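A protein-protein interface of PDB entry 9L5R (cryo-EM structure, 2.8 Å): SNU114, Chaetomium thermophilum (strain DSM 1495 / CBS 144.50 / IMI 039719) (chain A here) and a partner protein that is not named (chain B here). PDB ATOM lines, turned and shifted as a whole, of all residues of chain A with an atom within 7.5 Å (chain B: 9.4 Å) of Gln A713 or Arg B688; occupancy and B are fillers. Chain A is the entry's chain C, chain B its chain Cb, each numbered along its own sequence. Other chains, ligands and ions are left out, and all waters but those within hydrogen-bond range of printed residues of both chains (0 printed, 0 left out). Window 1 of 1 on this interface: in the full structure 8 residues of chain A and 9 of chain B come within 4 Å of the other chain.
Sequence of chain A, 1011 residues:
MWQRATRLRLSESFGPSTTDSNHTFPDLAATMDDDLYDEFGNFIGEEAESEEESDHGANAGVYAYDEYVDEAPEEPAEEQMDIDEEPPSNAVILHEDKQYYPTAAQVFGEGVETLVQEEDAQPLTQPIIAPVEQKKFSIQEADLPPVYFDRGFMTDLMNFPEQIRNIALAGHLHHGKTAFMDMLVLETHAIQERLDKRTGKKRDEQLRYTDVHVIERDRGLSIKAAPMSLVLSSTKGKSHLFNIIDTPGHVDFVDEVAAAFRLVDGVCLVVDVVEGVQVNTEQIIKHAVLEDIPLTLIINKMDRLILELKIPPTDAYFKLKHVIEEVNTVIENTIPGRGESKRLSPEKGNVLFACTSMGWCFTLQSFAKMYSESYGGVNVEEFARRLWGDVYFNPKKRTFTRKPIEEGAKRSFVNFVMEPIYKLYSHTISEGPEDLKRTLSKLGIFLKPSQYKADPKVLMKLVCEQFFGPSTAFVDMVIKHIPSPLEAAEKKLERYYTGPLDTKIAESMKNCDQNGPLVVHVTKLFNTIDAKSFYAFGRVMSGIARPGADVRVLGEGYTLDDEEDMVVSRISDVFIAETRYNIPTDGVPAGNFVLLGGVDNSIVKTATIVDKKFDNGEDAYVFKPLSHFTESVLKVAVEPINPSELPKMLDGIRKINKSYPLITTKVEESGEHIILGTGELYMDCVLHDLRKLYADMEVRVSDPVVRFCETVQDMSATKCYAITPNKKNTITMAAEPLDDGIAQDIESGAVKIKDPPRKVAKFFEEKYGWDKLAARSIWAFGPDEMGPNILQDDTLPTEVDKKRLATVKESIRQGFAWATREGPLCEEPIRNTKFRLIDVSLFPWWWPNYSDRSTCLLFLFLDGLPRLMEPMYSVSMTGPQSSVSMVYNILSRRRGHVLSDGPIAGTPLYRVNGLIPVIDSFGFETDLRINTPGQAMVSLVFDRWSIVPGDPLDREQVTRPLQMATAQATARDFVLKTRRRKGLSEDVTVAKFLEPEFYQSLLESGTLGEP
O of Arg B688 sits close to OD1 of Asp A714.
NE of Arg A867 sits at hydrogen-bond distance from O of Gly A950 (2.9 Å). NE2 of Gln A713 sits close to NH1 of Arg A867.
Among the printed residues, merely in contact across the chains: Gln A713 with Arg B688 (3.4 Å), Asp A714 with Thr B692 (3.4 Å), Met A715 with Asp B695 (3.7 Å), Met A715 with Ala B696 (3.9 Å), Gly A950 with Ala B679 (3.8 Å), Gly A950 with Thr B680 (3.4 Å) and Asp A951 with Ala B679 (3.4 Å).
No residue of chain B comes within 4 Å of Val A712. Gln A713 touches just one residue of chain B: Arg B688 (3.4 Å). Gly A864 touches none of the printed residues of chain B. Printed residues of chain B within 4 Å of Gly A950: Ala B679 and Thr B680. Of the printed residues of chain B, Asp A951 touches Ala B679 (3.4 Å). No residue of chain A comes within 4 Å of Arg B687. Of the printed residues of chain A, Arg B688 touches Gln A713 and Asp A714. The nearest residue of chain A that does not touch Arg B688 is Arg A867 (6.2 Å). The nearest printed residue of chain A that does not touch Thr B692 is Met A715 (4.5 Å).
Of the 29 printed residues of chain B, 6 touch a printed residue of chain A. Hydrophobic or aromatic side chains of chain B within 4 Å of the printed part of chain A: Ala B679 and Ala B696. Of the 18 printed residues of chain A, 5 touch a printed residue of chain B. Printed residues of chain A that touch a printed residue of chain B: Gln A713, Asp A714, Met A715, Gly A950 and Asp A951. Among the printed residues, 8 pairs touch across the chains.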
ATOM      1  N   THR A 711      21.207   8.563   7.529  1.00  0.00           N
ATOM      2  CA  THR A 711      20.901   7.258   8.109  1.00  0.00           C
ATOM      3  C   THR A 711      20.372   7.467   9.521  1.00  0.00           C
ATOM      4  O   THR A 711      20.288   8.592  10.009  1.00  0.00           O
ATOM      5  CB  THR A 711      22.130   6.347   8.122  1.00  0.00           C
ATOM      6  OG1 THR A 711      21.729   5.006   8.427  1.00  0.00           O
ATOM      7  CG2 THR A 711      23.127   6.824   9.162  1.00  0.00           C
ATOM      8  N   VAL A 712      20.017   6.365  10.181  1.00  0.00           N
ATOM      9  CA  VAL A 712      19.648   6.374  11.591  1.00  0.00           C
ATOM     10  C   VAL A 712      20.511   5.358  12.326  1.00  0.00           C
ATOM     11  O   VAL A 712      20.991   4.383  11.739  1.00  0.00           O
ATOM     12  CB  VAL A 712      18.148   6.074  11.797  1.00  0.00           C
ATOM     13  CG1 VAL A 712      17.296   7.140  11.135  1.00  0.00           C
ATOM     14  CG2 VAL A 712      17.796   4.714  11.234  1.00  0.00           C
ATOM     15  N   GLN A 713      20.729   5.603  13.620  1.00  0.00           N
ATOM     16  CA  GLN A 713      21.476   4.669  14.449  1.00  0.00           C
ATOM     17  C   GLN A 713      20.684   4.112  15.625  1.00  0.00           C
ATOM     18  O   GLN A 713      21.131   3.135  16.236  1.00  0.00           O
ATOM     19  CB  GLN A 713      22.768   5.314  14.976  1.00  0.00           C
ATOM     20  CG  GLN A 713      22.630   6.010  16.314  1.00  0.00           C
ATOM     21  CD  GLN A 713      23.831   6.863  16.645  1.00  0.00           C
ATOM     22  OE1 GLN A 713      24.634   7.185  15.773  1.00  0.00           O
ATOM     23  NE2 GLN A 713      23.961   7.238  17.910  1.00  0.00           N
ATOM     24  N   ASP A 714      19.524   4.678  15.945  1.00  0.00           N
ATOM     25  CA  ASP A 714      18.660   4.164  16.997  1.00  0.00           C
ATOM     26  C   ASP A 714      17.252   3.988  16.453  1.00  0.00           C
ATOM     27  O   ASP A 714      16.815   4.750  15.587  1.00  0.00           O
ATOM     28  CB  ASP A 714      18.633   5.098  18.215  1.00  0.00           C
ATOM     29  CG  ASP A 714      19.994   5.260  18.861  1.00  0.00           C
ATOM     30  OD1 ASP A 714      20.745   4.264  18.928  1.00  0.00           O
ATOM     31  OD2 ASP A 714      20.314   6.383  19.303  1.00  0.00           O
ATOM     32  N   MET A 715      16.549   2.982  16.963  1.00  0.00           N
ATOM     33  CA  MET A 715      15.178   2.741  16.544  1.00  0.00           C
ATOM     34  C   MET A 715      14.253   3.824  17.095  1.00  0.00           C
ATOM     35  O   MET A 715      14.551   4.488  18.091  1.00  0.00           O
ATOM     36  CB  MET A 715      14.737   1.336  16.975  1.00  0.00           C
ATOM     37  CG  MET A 715      14.740   1.040  18.480  1.00  0.00           C
ATOM     38  SD  MET A 715      13.346   1.650  19.455  1.00  0.00           S
ATOM     39  CE  MET A 715      12.039   0.570  18.879  1.00  0.00           C
ATOM     40  N   GLU A 736      13.808   2.270  11.965  1.00  0.00           N
ATOM     41  CA  GLU A 736      14.824   1.423  12.574  1.00  0.00           C
ATOM     42  C   GLU A 736      16.051   1.418  11.675  1.00  0.00           C
ATOM     43  O   GLU A 736      15.914   1.535  10.455  1.00  0.00           O
ATOM     44  CB  GLU A 736      14.287  -0.005  12.763  1.00  0.00           C
ATOM     45  CG  GLU A 736      15.206  -0.970  13.493  1.00  0.00           C
ATOM     46  CD  GLU A 736      14.666  -2.383  13.512  1.00  0.00           C
ATOM     47  OE1 GLU A 736      13.496  -2.576  13.121  1.00  0.00           O
ATOM     48  OE2 GLU A 736      15.414  -3.302  13.907  1.00  0.00           O
ATOM     49  N   PRO A 737      17.254   1.324  12.237  1.00  0.00           N
ATOM     50  CA  PRO A 737      18.426   1.045  11.402  1.00  0.00           C
ATOM     51  C   PRO A 737      18.368  -0.359  10.827  1.00  0.00           C
ATOM     52  O   PRO A 737      17.866  -1.293  11.455  1.00  0.00           O
ATOM     53  CB  PRO A 737      19.603   1.189  12.371  1.00  0.00           C
ATOM     54  CG  PRO A 737      19.084   1.980  13.490  1.00  0.00           C
ATOM     55  CD  PRO A 737      17.633   1.680  13.613  1.00  0.00           C
ATOM     56  N   ASN A 832      20.077   3.014   4.569  1.00  0.00           N
ATOM     57  CA  ASN A 832      20.150   2.074   5.688  1.00  0.00           C
ATOM     58  C   ASN A 832      19.001   2.294   6.675  1.00  0.00           C
ATOM     59  O   ASN A 832      19.204   2.585   7.854  1.00  0.00           O
ATOM     60  CB  ASN A 832      21.508   2.179   6.390  1.00  0.00           C
ATOM     61  CG  ASN A 832      22.063   0.837   6.786  1.00  0.00           C
ATOM     62  OD1 ASN A 832      21.670  -0.192   6.244  1.00  0.00           O
ATOM     63  ND2 ASN A 832      22.983   0.836   7.740  1.00  0.00           N
ATOM     64  N   PHE A 861      12.209  10.226  11.130  1.00  0.00           N
ATOM     65  CA  PHE A 861      13.670  10.224  11.114  1.00  0.00           C
ATOM     66  C   PHE A 861      14.230  11.011  12.291  1.00  0.00           C
ATOM     67  O   PHE A 861      15.172  10.564  12.964  1.00  0.00           O
ATOM     68  CB  PHE A 861      14.194  10.814   9.809  1.00  0.00           C
ATOM     69  CG  PHE A 861      13.960   9.946   8.625  1.00  0.00           C
ATOM     70  CD1 PHE A 861      14.220   8.593   8.685  1.00  0.00           C
ATOM     71  CD2 PHE A 861      13.514  10.494   7.433  1.00  0.00           C
ATOM     72  CE1 PHE A 861      14.000   7.794   7.591  1.00  0.00           C
ATOM     73  CE2 PHE A 861      13.304   9.706   6.330  1.00  0.00           C
ATOM     74  CZ  PHE A 861      13.554   8.357   6.402  1.00  0.00           C
ATOM     75  N   GLY A 864      13.957   9.041  15.196  1.00  0.00           N
ATOM     76  CA  GLY A 864      14.951   7.993  15.095  1.00  0.00           C
ATOM     77  C   GLY A 864      16.369   8.465  15.308  1.00  0.00           C
ATOM     78  O   GLY A 864      17.284   7.633  15.296  1.00  0.00           O
ATOM     79  N   LEU A 865      16.565   9.781  15.488  1.00  0.00           N
ATOM     80  CA  LEU A 865      17.836  10.409  15.855  1.00  0.00           C
ATOM     81  C   LEU A 865      18.892  10.160  14.785  1.00  0.00           C
ATOM     82  O   LEU A 865      19.818   9.366  14.987  1.00  0.00           O
ATOM     83  CB  LEU A 865      18.320   9.912  17.220  1.00  0.00           C
ATOM     84  CG  LEU A 865      17.315  10.082  18.361  1.00  0.00           C
ATOM     85  CD1 LEU A 865      17.869   9.522  19.661  1.00  0.00           C
ATOM     86  CD2 LEU A 865      16.926  11.544  18.522  1.00  0.00           C
ATOM     87  N   PRO A 866      18.778  10.827  13.642  1.00  0.00           N
ATOM     88  CA  PRO A 866      19.557  10.447  12.465  1.00  0.00           C
ATOM     89  C   PRO A 866      21.014  10.878  12.569  1.00  0.00           C
ATOM     90  O   PRO A 866      21.424  11.616  13.465  1.00  0.00           O
ATOM     91  CB  PRO A 866      18.842  11.193  11.338  1.00  0.00           C
ATOM     92  CG  PRO A 866      18.359  12.434  11.993  1.00  0.00           C
ATOM     93  CD  PRO A 866      18.032  12.078  13.421  1.00  0.00           C
ATOM     94  N   ARG A 867      21.795  10.377  11.617  1.00  0.00           N
ATOM     95  CA  ARG A 867      23.201  10.698  11.451  1.00  0.00           C
ATOM     96  C   ARG A 867      23.479  10.949   9.978  1.00  0.00           C
ATOM     97  O   ARG A 867      22.735  10.510   9.095  1.00  0.00           O
ATOM     98  CB  ARG A 867      24.108   9.575  11.955  1.00  0.00           C
ATOM     99  CG  ARG A 867      23.992   9.293  13.430  1.00  0.00           C
ATOM    100  CD  ARG A 867      24.491  10.457  14.250  1.00  0.00           C
ATOM    101  NE  ARG A 867      25.947  10.534  14.262  1.00  0.00           N
ATOM    102  CZ  ARG A 867      26.732   9.808  15.046  1.00  0.00           C
ATOM    103  NH1 ARG A 867      26.236   8.930  15.900  1.00  0.00           N
ATOM    104  NH2 ARG A 867      28.050   9.971  14.973  1.00  0.00           N
ATOM    105  N   ILE A 947      29.871   6.717   8.645  1.00  0.00           N
ATOM    106  CA  ILE A 947      29.260   7.708   9.521  1.00  0.00           C
ATOM    107  C   ILE A 947      30.260   8.824   9.778  1.00  0.00           C
ATOM    108  O   ILE A 947      31.388   8.571  10.213  1.00  0.00           O
ATOM    109  CB  ILE A 947      28.819   7.062  10.842  1.00  0.00           C
ATOM    110  CG1 ILE A 947      27.945   5.840  10.577  1.00  0.00           C
ATOM    111  CG2 ILE A 947      28.069   8.061  11.694  1.00  0.00           C
ATOM    112  CD1 ILE A 947      26.660   6.158   9.897  1.00  0.00           C
ATOM    113  N   VAL A 948      29.855  10.058   9.517  1.00  0.00           N
ATOM    114  CA  VAL A 948      30.720  11.188   9.868  1.00  0.00           C
ATOM    115  C   VAL A 948      30.715  11.365  11.382  1.00  0.00           C
ATOM    116  O   VAL A 948      29.673  11.136  12.024  1.00  0.00           O
ATOM    117  CB  VAL A 948      30.266  12.459   9.132  1.00  0.00           C
ATOM    118  CG1 VAL A 948      28.886  12.876   9.531  1.00  0.00           C
ATOM    119  CG2 VAL A 948      31.226  13.601   9.363  1.00  0.00           C
ATOM    120  N   GLY A 950      30.374  12.970  14.991  1.00  0.00           N
ATOM    121  CA  GLY A 950      29.533  14.016  15.527  1.00  0.00           C
ATOM    122  C   GLY A 950      28.056  13.720  15.321  1.00  0.00           C
ATOM    123  O   GLY A 950      27.660  12.881  14.507  1.00  0.00           O
ATOM    124  N   ASP A 951      27.231  14.428  16.088  1.00  0.00           N
ATOM    125  CA  ASP A 951      25.789  14.334  15.968  1.00  0.00           C
ATOM    126  C   ASP A 951      25.265  15.559  15.245  1.00  0.00           C
ATOM    127  O   ASP A 951      25.573  16.686  15.651  1.00  0.00           O
ATOM    128  CB  ASP A 951      25.134  14.218  17.348  1.00  0.00           C
ATOM    129  CG  ASP A 951      23.842  13.420  17.317  1.00  0.00           C
ATOM    130  OD1 ASP A 951      22.873  13.877  16.679  1.00  0.00           O
ATOM    131  OD2 ASP A 951      23.798  12.332  17.931  1.00  0.00           O
ATOM    132  N   PRO A 952      24.496  15.383  14.167  1.00  0.00           N
ATOM    133  CA  PRO A 952      24.081  16.540  13.360  1.00  0.00           C
ATOM    134  C   PRO A 952      23.113  17.476  14.057  1.00  0.00           C
ATOM    135  O   PRO A 952      22.969  18.622  13.614  1.00  0.00           O
ATOM    136  CB  PRO A 952      23.427  15.889  12.137  1.00  0.00           C
ATOM    137  CG  PRO A 952      22.975  14.571  12.623  1.00  0.00           C
ATOM    138  CD  PRO A 952      24.008  14.118  13.604  1.00  0.00           C
ATOM    139  N   VAL B 645      32.406  -1.670  18.402  1.00  0.00           N
ATOM    140  CA  VAL B 645      31.188  -1.226  19.075  1.00  0.00           C
ATOM    141  C   VAL B 645      30.099  -0.893  18.062  1.00  0.00           C
ATOM    142  O   VAL B 645      28.912  -1.145  18.302  1.00  0.00           O
ATOM    143  CB  VAL B 645      31.491  -0.027  19.990  1.00  0.00           C
ATOM    144  N   GLU B 646      30.479  -0.316  16.920  1.00  0.00           N
ATOM    145  CA  GLU B 646      29.489   0.020  15.902  1.00  0.00           C
ATOM    146  C   GLU B 646      28.996  -1.222  15.171  1.00  0.00           C
ATOM    147  O   GLU B 646      27.806  -1.325  14.850  1.00  0.00           O
ATOM    148  CB  GLU B 646      30.075   1.027  14.913  1.00  0.00           C
ATOM    149  N   TRP B 648      29.029  -4.472  16.299  1.00  0.00           N
ATOM    150  CA  TRP B 648      28.380  -5.463  17.147  1.00  0.00           C
ATOM    151  C   TRP B 648      26.927  -5.079  17.405  1.00  0.00           C
ATOM    152  O   TRP B 648      26.630  -3.937  17.770  1.00  0.00           O
ATOM    153  CB  TRP B 648      29.131  -5.607  18.470  1.00  0.00           C
ATOM    154  N   PRO B 650      23.793  -4.841  19.582  1.00  0.00           N
ATOM    155  CA  PRO B 650      23.525  -4.905  21.028  1.00  0.00           C
ATOM    156  C   PRO B 650      22.485  -5.943  21.413  1.00  0.00           C
ATOM    157  O   PRO B 650      22.577  -6.517  22.505  1.00  0.00           O
ATOM    158  CB  PRO B 650      23.051  -3.483  21.359  1.00  0.00           C
ATOM    159  N   ALA B 676      31.630  10.648  27.887  1.00  0.00           N
ATOM    160  CA  ALA B 676      30.272  10.229  27.562  1.00  0.00           C
ATOM    161  C   ALA B 676      29.452  11.377  26.991  1.00  0.00           C
ATOM    162  O   ALA B 676      28.494  11.141  26.245  1.00  0.00           O
ATOM    163  CB  ALA B 676      29.589   9.652  28.801  1.00  0.00           C
ATOM    164  N   ALA B 678      30.481  13.440  24.812  1.00  0.00           N
ATOM    165  CA  ALA B 678      30.892  13.693  23.439  1.00  0.00           C
ATOM    166  C   ALA B 678      29.854  13.170  22.455  1.00  0.00           C
ATOM    167  O   ALA B 678      29.112  12.228  22.749  1.00  0.00           O
ATOM    168  CB  ALA B 678      32.248  13.045  23.164  1.00  0.00           C
ATOM    169  N   ALA B 679      29.789  13.809  21.283  1.00  0.00           N
ATOM    170  CA  ALA B 679      28.881  13.352  20.236  1.00  0.00           C
ATOM    171  C   ALA B 679      29.421  12.120  19.521  1.00  0.00           C
ATOM    172  O   ALA B 679      28.639  11.273  19.073  1.00  0.00           O
ATOM    173  CB  ALA B 679      28.626  14.477  19.234  1.00  0.00           C
ATOM    174  N   THR B 680      30.740  12.007  19.396  1.00  0.00           N
ATOM    175  CA  THR B 680      31.384  10.871  18.752  1.00  0.00           C
ATOM    176  C   THR B 680      32.443  10.303  19.682  1.00  0.00           C
ATOM    177  O   THR B 680      33.163  11.057  20.345  1.00  0.00           O
ATOM    178  CB  THR B 680      32.018  11.273  17.418  1.00  0.00           C
ATOM    179  N   GLY B 681      32.536   8.984  19.728  1.00  0.00           N
ATOM    180  CA  GLY B 681      33.515   8.329  20.571  1.00  0.00           C
ATOM    181  C   GLY B 681      33.070   6.934  20.926  1.00  0.00           C
ATOM    182  O   GLY B 681      31.945   6.519  20.645  1.00  0.00           O
ATOM    183  N   LEU B 682      33.993   6.197  21.548  1.00  0.00           N
ATOM    184  CA  LEU B 682      33.672   4.854  22.022  1.00  0.00           C
ATOM    185  C   LEU B 682      32.623   4.898  23.127  1.00  0.00           C
ATOM    186  O   LEU B 682      31.678   4.102  23.126  1.00  0.00           O
ATOM    187  CB  LEU B 682      34.939   4.155  22.511  1.00  0.00           C
ATOM    188  N   VAL B 683      32.762   5.842  24.061  1.00  0.00           N
ATOM    189  CA  VAL B 683      31.798   5.972  25.151  1.00  0.00           C
ATOM    190  C   VAL B 683      30.448   6.441  24.623  1.00  0.00           C
ATOM    191  O   VAL B 683      29.396   5.977  25.078  1.00  0.00           O
ATOM    192  CB  VAL B 683      32.342   6.919  26.235  1.00  0.00           C
ATOM    193  N   ALA B 684      30.455   7.370  23.662  1.00  0.00           N
ATOM    194  CA  ALA B 684      29.208   7.837  23.062  1.00  0.00           C
ATOM    195  C   ALA B 684      28.507   6.723  22.295  1.00  0.00           C
ATOM    196  O   ALA B 684      27.280   6.589  22.370  1.00  0.00           O
ATOM    197  CB  ALA B 684      29.481   9.027  22.145  1.00  0.00           C
ATOM    198  N   ASP B 685      29.273   5.912  21.559  1.00  0.00           N
ATOM    199  CA  ASP B 685      28.694   4.777  20.847  1.00  0.00           C
ATOM    200  C   ASP B 685      28.143   3.737  21.814  1.00  0.00           C
ATOM    201  O   ASP B 685      27.089   3.147  21.558  1.00  0.00           O
ATOM    202  CB  ASP B 685      29.737   4.151  19.922  1.00  0.00           C
ATOM    203  N   VAL B 686      28.841   3.504  22.930  1.00  0.00           N
ATOM    204  CA  VAL B 686      28.360   2.555  23.929  1.00  0.00           C
ATOM    205  C   VAL B 686      27.074   3.055  24.576  1.00  0.00           C
ATOM    206  O   VAL B 686      26.137   2.280  24.801  1.00  0.00           O
ATOM    207  CB  VAL B 686      29.453   2.286  24.979  1.00  0.00           C
ATOM    208  N   ARG B 687      27.008   4.354  24.885  1.00  0.00           N
ATOM    209  CA  ARG B 687      25.795   4.925  25.466  1.00  0.00           C
ATOM    210  C   ARG B 687      24.628   4.874  24.488  1.00  0.00           C
ATOM    211  O   ARG B 687      23.495   4.573  24.882  1.00  0.00           O
ATOM    212  CB  ARG B 687      26.057   6.363  25.916  1.00  0.00           C
ATOM    213  N   ARG B 688      24.885   5.162  23.207  1.00  0.00           N
ATOM    214  CA  ARG B 688      23.833   5.082  22.197  1.00  0.00           C
ATOM    215  C   ARG B 688      23.355   3.647  21.999  1.00  0.00           C
ATOM    216  O   ARG B 688      22.154   3.406  21.838  1.00  0.00           O
ATOM    217  CB  ARG B 688      24.329   5.671  20.877  1.00  0.00           C
ATOM    218  N   LYS B 689      24.282   2.682  22.010  1.00  0.00           N
ATOM    219  CA  LYS B 689      23.901   1.278  21.896  1.00  0.00           C
ATOM    220  C   LYS B 689      23.096   0.822  23.106  1.00  0.00           C
ATOM    221  O   LYS B 689      22.131   0.063  22.962  1.00  0.00           O
ATOM    222  CB  LYS B 689      25.147   0.409  21.721  1.00  0.00           C
ATOM    223  N   PHE B 690      23.475   1.278  24.304  1.00  0.00           N
ATOM    224  CA  PHE B 690      22.720   0.939  25.507  1.00  0.00           C
ATOM    225  C   PHE B 690      21.325   1.552  25.477  1.00  0.00           C
ATOM    226  O   PHE B 690      20.352   0.908  25.881  1.00  0.00           O
ATOM    227  CB  PHE B 690      23.482   1.397  26.749  1.00  0.00           C
ATOM    228  N   ARG B 691      21.210   2.794  24.994  1.00  0.00           N
ATOM    229  CA  ARG B 691      19.901   3.428  24.866  1.00  0.00           C
ATOM    230  C   ARG B 691      19.032   2.709  23.839  1.00  0.00           C
ATOM    231  O   ARG B 691      17.830   2.520  24.061  1.00  0.00           O
ATOM    232  CB  ARG B 691      20.067   4.901  24.492  1.00  0.00           C
ATOM    233  N   THR B 692      19.623   2.297  22.713  1.00  0.00           N
ATOM    234  CA  THR B 692      18.872   1.557  21.702  1.00  0.00           C
ATOM    235  C   THR B 692      18.423   0.197  22.227  1.00  0.00           C
ATOM    236  O   THR B 692      17.295  -0.235  21.960  1.00  0.00           O
ATOM    237  CB  THR B 692      19.713   1.390  20.436  1.00  0.00           C
ATOM    238  N   LEU B 693      19.294  -0.489  22.975  1.00  0.00           N
ATOM    239  CA  LEU B 693      18.927  -1.775  23.560  1.00  0.00           C
ATOM    240  C   LEU B 693      17.848  -1.613  24.622  1.00  0.00           C
ATOM    241  O   LEU B 693      16.967  -2.468  24.752  1.00  0.00           O
ATOM    242  CB  LEU B 693      20.163  -2.455  24.149  1.00  0.00           C
ATOM    243  N   ILE B 694      17.898  -0.521  25.388  1.00  0.00           N
ATOM    244  CA  ILE B 694      16.865  -0.261  26.384  1.00  0.00           C
ATOM    245  C   ILE B 694      15.537   0.059  25.706  1.00  0.00           C
ATOM    246  O   ILE B 694      14.468  -0.327  26.193  1.00  0.00           O
ATOM    247  CB  ILE B 694      17.311   0.873  27.323  1.00  0.00           C
ATOM    248  N   ASP B 695      15.582   0.773  24.579  1.00  0.00           N
ATOM    249  CA  ASP B 695      14.357   1.115  23.862  1.00  0.00           C
ATOM    250  C   ASP B 695      13.740  -0.107  23.193  1.00  0.00           C
ATOM    251  O   ASP B 695      12.512  -0.265  23.190  1.00  0.00           O
ATOM    252  CB  ASP B 695      14.644   2.204  22.829  1.00  0.00           C
ATOM    253  N   ALA B 696      14.565  -0.984  22.620  1.00  0.00           N
ATOM    254  CA  ALA B 696      14.084  -2.163  21.909  1.00  0.00           C
ATOM    255  C   ALA B 696      14.323  -3.450  22.695  1.00  0.00           C
ATOM    256  O   ALA B 696      14.504  -4.518  22.105  1.00  0.00           O
ATOM    257  CB  ALA B 696      14.733  -2.255  20.529  1.00  0.00           C
ATOM    258  N   TRP B 710      29.002  -0.269  31.542  1.00  0.00           N
ATOM    259  CA  TRP B 710      28.824   0.874  30.649  1.00  0.00           C
ATOM    260  C   TRP B 710      28.341   2.103  31.412  1.00  0.00           C
ATOM    261  O   TRP B 710      28.830   3.215  31.185  1.00  0.00           O
ATOM    262  CB  TRP B 710      27.847   0.517  29.530  1.00  0.00           C
ATOM    263  N   LEU B 714      30.258   5.605  31.965  1.00  0.00           N
ATOM    264  CA  LEU B 714      29.619   6.810  31.453  1.00  0.00           C
ATOM    265  C   LEU B 714      28.975   7.666  32.536  1.00  0.00           C
ATOM    266  O   LEU B 714      28.365   8.690  32.211  1.00  0.00           O
ATOM    267  CB  LEU B 714      28.566   6.436  30.405  1.00  0.00           C
ATOM    268  N   TYR B 724      25.492  11.403  31.639  1.00  0.00           N
ATOM    269  CA  TYR B 724      24.711  10.877  30.529  1.00  0.00           C
ATOM    270  C   TYR B 724      24.142   9.493  30.804  1.00  0.00           C
ATOM    271  O   TYR B 724      23.520   8.906  29.914  1.00  0.00           O
ATOM    272  CB  TYR B 724      25.565  10.837  29.257  1.00  0.00           C
ATOM    273  N   LEU B 728      19.635   9.061  30.105  1.00  0.00           N
ATOM    274  CA  LEU B 728      19.364   8.126  29.016  1.00  0.00           C
ATOM    275  C   LEU B 728      18.650   6.880  29.523  1.00  0.00           C
ATOM    276  O   LEU B 728      17.738   6.367  28.863  1.00  0.00           O
ATOM    277  CB  LEU B 728      20.667   7.750  28.312  1.00  0.00           C
ATOM    278  N   HIS B 732      14.919   5.833  28.349  1.00  0.00           N
ATOM    279  CA  HIS B 732      14.814   4.676  27.469  1.00  0.00           C
ATOM    280  C   HIS B 732      14.339   3.421  28.193  1.00  0.00           C
ATOM    281  O   HIS B 732      13.342   2.820  27.788  1.00  0.00           O
ATOM    282  CB  HIS B 732      16.166   4.420  26.788  1.00  0.00           C
